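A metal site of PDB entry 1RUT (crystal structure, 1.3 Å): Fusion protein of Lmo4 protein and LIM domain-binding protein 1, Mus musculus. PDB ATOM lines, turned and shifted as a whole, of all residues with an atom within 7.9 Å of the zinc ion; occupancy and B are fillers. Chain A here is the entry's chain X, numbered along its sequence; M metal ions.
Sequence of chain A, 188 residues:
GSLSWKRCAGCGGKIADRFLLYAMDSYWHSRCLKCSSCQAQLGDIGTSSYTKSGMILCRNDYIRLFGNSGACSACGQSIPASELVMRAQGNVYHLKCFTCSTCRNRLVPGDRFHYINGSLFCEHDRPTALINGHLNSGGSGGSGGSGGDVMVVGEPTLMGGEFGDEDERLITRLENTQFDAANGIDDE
The nearest printed residue that does not touch the zinc ion is Thr 102 (4.6 Å).
The zinc ion is bound by the side-chain carboxylate (OD2) of Asp 125 (2.0 Å), the side-chain sulfur (SG) of Cys 122 (2.3 Å), the side-chain sulfur (SG) of Cys 103 (2.3 Å) and the side-chain sulfur (SG) of Cys 100 (2.3 Å). The zinc ion has four donor atoms within binding distance.
SG of Cys 122 sits close to N of His 124 (3.6 Å). The backbone NH (N) of Asn 105 sits close to the side-chain sulfur (SG) of Cys 103 (3.5 Å). N of Thr 102 lies close to SG of Cys 100. N of Cys 100 is in hydrogen-bond range of O of Asn 105 (2.8 Å).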
ATOM      1  N   THR A  99     -10.399 -20.374  -8.107  1.00  0.00           N
ATOM      2  CA  THR A  99     -11.688 -20.270  -8.777  1.00  0.00           C
ATOM      3  C   THR A  99     -11.745 -21.081 -10.076  1.00  0.00           C
ATOM      4  O   THR A  99     -10.724 -21.339 -10.723  1.00  0.00           O
ATOM      5  CB  THR A  99     -12.027 -18.816  -9.136  1.00  0.00           C
ATOM      6  OG1 THR A  99     -10.973 -18.241  -9.926  1.00  0.00           O
ATOM      7  CG2 THR A  99     -12.123 -17.949  -7.889  1.00  0.00           C
ATOM      8  N   CYS A 100     -12.962 -21.448 -10.462  1.00  0.00           N
ATOM      9  CA  CYS A 100     -13.185 -22.087 -11.748  1.00  0.00           C
ATOM     10  C   CYS A 100     -12.937 -21.090 -12.883  1.00  0.00           C
ATOM     11  O   CYS A 100     -13.471 -19.983 -12.883  1.00  0.00           O
ATOM     12  CB  CYS A 100     -14.617 -22.630 -11.821  1.00  0.00           C
ATOM     13  SG  CYS A 100     -15.011 -23.346 -13.428  1.00  0.00           S
ATOM     14  N   SER A 101     -12.138 -21.506 -13.854  1.00  0.00           N
ATOM     15  CA  SER A 101     -11.767 -20.657 -14.985  1.00  0.00           C
ATOM     16  C   SER A 101     -12.940 -20.339 -15.913  1.00  0.00           C
ATOM     17  O   SER A 101     -12.901 -19.357 -16.662  1.00  0.00           O
ATOM     18  CB  SER A 101     -10.659 -21.334 -15.790  1.00  0.00           C
ATOM     19  OG  SER A 101      -9.466 -21.431 -15.032  1.00  0.00           O
ATOM     20  N   THR A 102     -13.972 -21.176 -15.897  1.00  0.00           N
ATOM     21  CA  THR A 102     -15.156 -20.981 -16.730  1.00  0.00           C
ATOM     22  C   THR A 102     -16.218 -20.127 -16.034  1.00  0.00           C
ATOM     23  O   THR A 102     -16.618 -19.083 -16.555  1.00  0.00           O
ATOM     24  CB  THR A 102     -15.745 -22.365 -17.103  1.00  0.00           C
ATOM     25  OG1 THR A 102     -14.758 -23.140 -17.795  1.00  0.00           O
ATOM     26  CG2 THR A 102     -16.917 -22.244 -18.085  1.00  0.00           C
ATOM     27  N   CYS A 103     -16.674 -20.563 -14.863  1.00  0.00           N
ATOM     28  CA  CYS A 103     -17.805 -19.917 -14.190  1.00  0.00           C
ATOM     29  C   CYS A 103     -17.417 -18.935 -13.100  1.00  0.00           C
ATOM     30  O   CYS A 103     -18.263 -18.188 -12.634  1.00  0.00           O
ATOM     31  CB  CYS A 103     -18.778 -20.963 -13.633  1.00  0.00           C
ATOM     32  SG  CYS A 103     -18.230 -21.866 -12.178  1.00  0.00           S
ATOM     33  N   ARG A 104     -16.155 -18.956 -12.681  1.00  0.00           N
ATOM     34  CA  ARG A 104     -15.607 -18.057 -11.654  1.00  0.00           C
ATOM     35  C   ARG A 104     -15.986 -18.424 -10.214  1.00  0.00           C
ATOM     36  O   ARG A 104     -15.608 -17.729  -9.286  1.00  0.00           O
ATOM     37  CB  ARG A 104     -15.958 -16.588 -11.927  1.00  0.00           C
ATOM     38  CG  ARG A 104     -15.542 -16.083 -13.315  1.00  0.00           C
ATOM     39  CD  ARG A 104     -15.812 -14.597 -13.520  1.00  0.00           C
ATOM     40  NE  ARG A 104     -15.001 -13.753 -12.635  1.00  0.00           N
ATOM     41  CZ  ARG A 104     -13.704 -13.482 -12.813  1.00  0.00           C
ATOM     42  NH1 ARG A 104     -13.033 -13.984 -13.850  1.00  0.00           N
ATOM     43  NH2 ARG A 104     -13.074 -12.706 -11.947  1.00  0.00           N
ATOM     44  N   ASN A 105     -16.683 -19.547 -10.003  1.00  0.00           N
ATOM     45  CA  ASN A 105     -16.964 -19.994  -8.640  1.00  0.00           C
ATOM     46  C   ASN A 105     -15.681 -20.261  -7.863  1.00  0.00           C
ATOM     47  O   ASN A 105     -14.749 -20.881  -8.361  1.00  0.00           O
ATOM     48  CB  ASN A 105     -17.779 -21.287  -8.641  1.00  0.00           C
ATOM     49  CG  ASN A 105     -19.274 -21.065  -8.660  1.00  0.00           C
ATOM     50  OD1 ASN A 105     -19.762 -20.026  -9.094  1.00  0.00           O
ATOM     51  ND2 ASN A 105     -20.013 -22.067  -8.203  1.00  0.00           N
ATOM     52  N   ARG A 106     -15.654 -19.807  -6.618  1.00  0.00           N
ATOM     53  CA  ARG A 106     -14.595 -20.171  -5.681  1.00  0.00           C
ATOM     54  C   ARG A 106     -14.752 -21.637  -5.290  1.00  0.00           C
ATOM     55  O   ARG A 106     -15.835 -22.061  -4.881  1.00  0.00           O
ATOM     56  CB  ARG A 106     -14.681 -19.289  -4.446  1.00  0.00           C
ATOM     57  CG  ARG A 106     -13.494 -19.384  -3.528  1.00  0.00           C
ATOM     58  CD  ARG A 106     -13.599 -18.479  -2.325  1.00  0.00           C
ATOM     59  NE  ARG A 106     -14.089 -17.152  -2.699  1.00  0.00           N
ATOM     60  CZ  ARG A 106     -14.853 -16.348  -1.940  1.00  0.00           C
ATOM     61  NH1 ARG A 106     -15.227 -16.711  -0.720  1.00  0.00           N
ATOM     62  NH2 ARG A 106     -15.235 -15.170  -2.420  1.00  0.00           N
ATOM     63  N   LEU A 107     -13.673 -22.385  -5.444  1.00  0.00           N
ATOM     64  CA  LEU A 107     -13.632 -23.796  -5.087  1.00  0.00           C
ATOM     65  C   LEU A 107     -13.268 -23.942  -3.615  1.00  0.00           C
ATOM     66  O   LEU A 107     -12.395 -23.231  -3.103  1.00  0.00           O
ATOM     67  CB  LEU A 107     -12.618 -24.538  -5.949  1.00  0.00           C
ATOM     68  CG  LEU A 107     -12.884 -24.439  -7.449  1.00  0.00           C
ATOM     69  CD1 LEU A 107     -11.691 -24.914  -8.239  1.00  0.00           C
ATOM     70  CD2 LEU A 107     -14.132 -25.231  -7.841  1.00  0.00           C
ATOM     71  N   LEU A 120      -7.982 -24.067 -13.569  1.00  0.00           N
ATOM     72  CA  LEU A 120      -8.842 -24.822 -12.672  1.00  0.00           C
ATOM     73  C   LEU A 120     -10.251 -24.816 -13.254  1.00  0.00           C
ATOM     74  O   LEU A 120     -10.686 -23.801 -13.805  1.00  0.00           O
ATOM     75  CB  LEU A 120      -8.878 -24.151 -11.297  1.00  0.00           C
ATOM     76  CG  LEU A 120      -7.538 -24.043 -10.571  1.00  0.00           C
ATOM     77  CD1 LEU A 120      -7.540 -22.917  -9.537  1.00  0.00           C
ATOM     78  CD2 LEU A 120      -7.211 -25.373  -9.924  1.00  0.00           C
ATOM     79  N   PHE A 121     -10.954 -25.934 -13.113  1.00  0.00           N
ATOM     80  CA  PHE A 121     -12.337 -26.045 -13.575  1.00  0.00           C
ATOM     81  C   PHE A 121     -13.146 -26.804 -12.538  1.00  0.00           C
ATOM     82  O   PHE A 121     -12.705 -27.823 -12.048  1.00  0.00           O
ATOM     83  CB  PHE A 121     -12.401 -26.787 -14.917  1.00  0.00           C
ATOM     84  CG  PHE A 121     -11.669 -26.099 -16.018  1.00  0.00           C
ATOM     85  CD1 PHE A 121     -12.281 -25.083 -16.733  1.00  0.00           C
ATOM     86  CD2 PHE A 121     -10.364 -26.443 -16.329  1.00  0.00           C
ATOM     87  CE1 PHE A 121     -11.608 -24.424 -17.743  1.00  0.00           C
ATOM     88  CE2 PHE A 121      -9.677 -25.784 -17.359  1.00  0.00           C
ATOM     89  CZ  PHE A 121     -10.310 -24.781 -18.058  1.00  0.00           C
ATOM     90  N   CYS A 122     -14.326 -26.309 -12.217  1.00  0.00           N
ATOM     91  CA  CYS A 122     -15.205 -27.002 -11.282  1.00  0.00           C
ATOM     92  C   CYS A 122     -15.806 -28.250 -11.934  1.00  0.00           C
ATOM     93  O   CYS A 122     -15.700 -28.458 -13.145  1.00  0.00           O
ATOM     94  CB  CYS A 122     -16.302 -26.069 -10.773  1.00  0.00           C
ATOM     95  SG  CYS A 122     -17.645 -25.777 -11.955  1.00  0.00           S
ATOM     96  N   GLU A 123     -16.451 -29.065 -11.103  1.00  0.00           N
ATOM     97  CA  GLU A 123     -17.027 -30.333 -11.534  1.00  0.00           C
ATOM     98  C   GLU A 123     -17.977 -30.199 -12.719  1.00  0.00           C
ATOM     99  O   GLU A 123     -18.050 -31.090 -13.562  1.00  0.00           O
ATOM    100  CB  GLU A 123     -17.778 -30.974 -10.354  1.00  0.00           C
ATOM    101  CG  GLU A 123     -18.200 -32.406 -10.626  1.00  0.00           C
ATOM    102  CD  GLU A 123     -18.906 -33.053  -9.445  1.00  0.00           C
ATOM    103  OE1 GLU A 123     -19.035 -32.411  -8.380  1.00  0.00           O
ATOM    104  OE2 GLU A 123     -19.343 -34.214  -9.597  1.00  0.00           O
ATOM    105  N   HIS A 124     -18.719 -29.102 -12.765  1.00  0.00           N
ATOM    106  CA  HIS A 124     -19.747 -28.893 -13.774  1.00  0.00           C
ATOM    107  C   HIS A 124     -19.278 -28.100 -14.978  1.00  0.00           C
ATOM    108  O   HIS A 124     -20.052 -27.795 -15.876  1.00  0.00           O
ATOM    109  CB  HIS A 124     -20.963 -28.274 -13.091  1.00  0.00           C
ATOM    110  CG  HIS A 124     -21.404 -29.058 -11.907  1.00  0.00           C
ATOM    111  ND1 HIS A 124     -21.895 -30.343 -12.010  1.00  0.00           N
ATOM    112  CD2 HIS A 124     -21.354 -28.781 -10.580  1.00  0.00           C
ATOM    113  CE1 HIS A 124     -22.174 -30.804 -10.810  1.00  0.00           C
ATOM    114  NE2 HIS A 124     -21.849 -29.875  -9.919  1.00  0.00           N
ATOM    115  N   ASP A 125     -17.992 -27.779 -14.988  1.00  0.00           N
ATOM    116  CA  ASP A 125     -17.328 -27.141 -16.129  1.00  0.00           C
ATOM    117  C   ASP A 125     -16.135 -27.959 -16.588  1.00  0.00           C
ATOM    118  O   ASP A 125     -15.099 -27.415 -16.963  1.00  0.00           O
ATOM    119  CB  ASP A 125     -16.891 -25.718 -15.767  1.00  0.00           C
ATOM    120  CG  ASP A 125     -18.052 -24.762 -15.696  1.00  0.00           C
ATOM    121  OD1 ASP A 125     -18.899 -24.791 -16.608  1.00  0.00           O
ATOM    122  OD2 ASP A 125     -18.207 -23.969 -14.750  1.00  0.00           O
ATOM    123  N   ARG A 126     -16.287 -29.286 -16.569  1.00  0.00           N
ATOM    124  CA  ARG A 126     -15.288 -30.188 -17.141  1.00  0.00           C
ATOM    125  C   ARG A 126     -15.010 -29.700 -18.565  1.00  0.00           C
ATOM    126  O   ARG A 126     -15.928 -29.608 -19.370  1.00  0.00           O
ATOM    127  CB  ARG A 126     -15.820 -31.623 -17.147  1.00  0.00           C
ATOM    128  CG  ARG A 126     -14.865 -32.676 -17.703  1.00  0.00           C
ATOM    129  CD  ARG A 126     -15.522 -34.053 -17.849  1.00  0.00           C
ATOM    130  NE  ARG A 126     -14.547 -35.112 -18.127  1.00  0.00           N
ATOM    131  CZ  ARG A 126     -14.077 -35.429 -19.340  1.00  0.00           C
ATOM    132  NH1 ARG A 126     -14.453 -34.755 -20.420  1.00  0.00           N
ATOM    133  NH2 ARG A 126     -13.200 -36.426 -19.451  1.00  0.00           N
HETATM  134 ZN    ZN M   1     -17.280 -23.790 -13.012  1.00  0.00          ZN
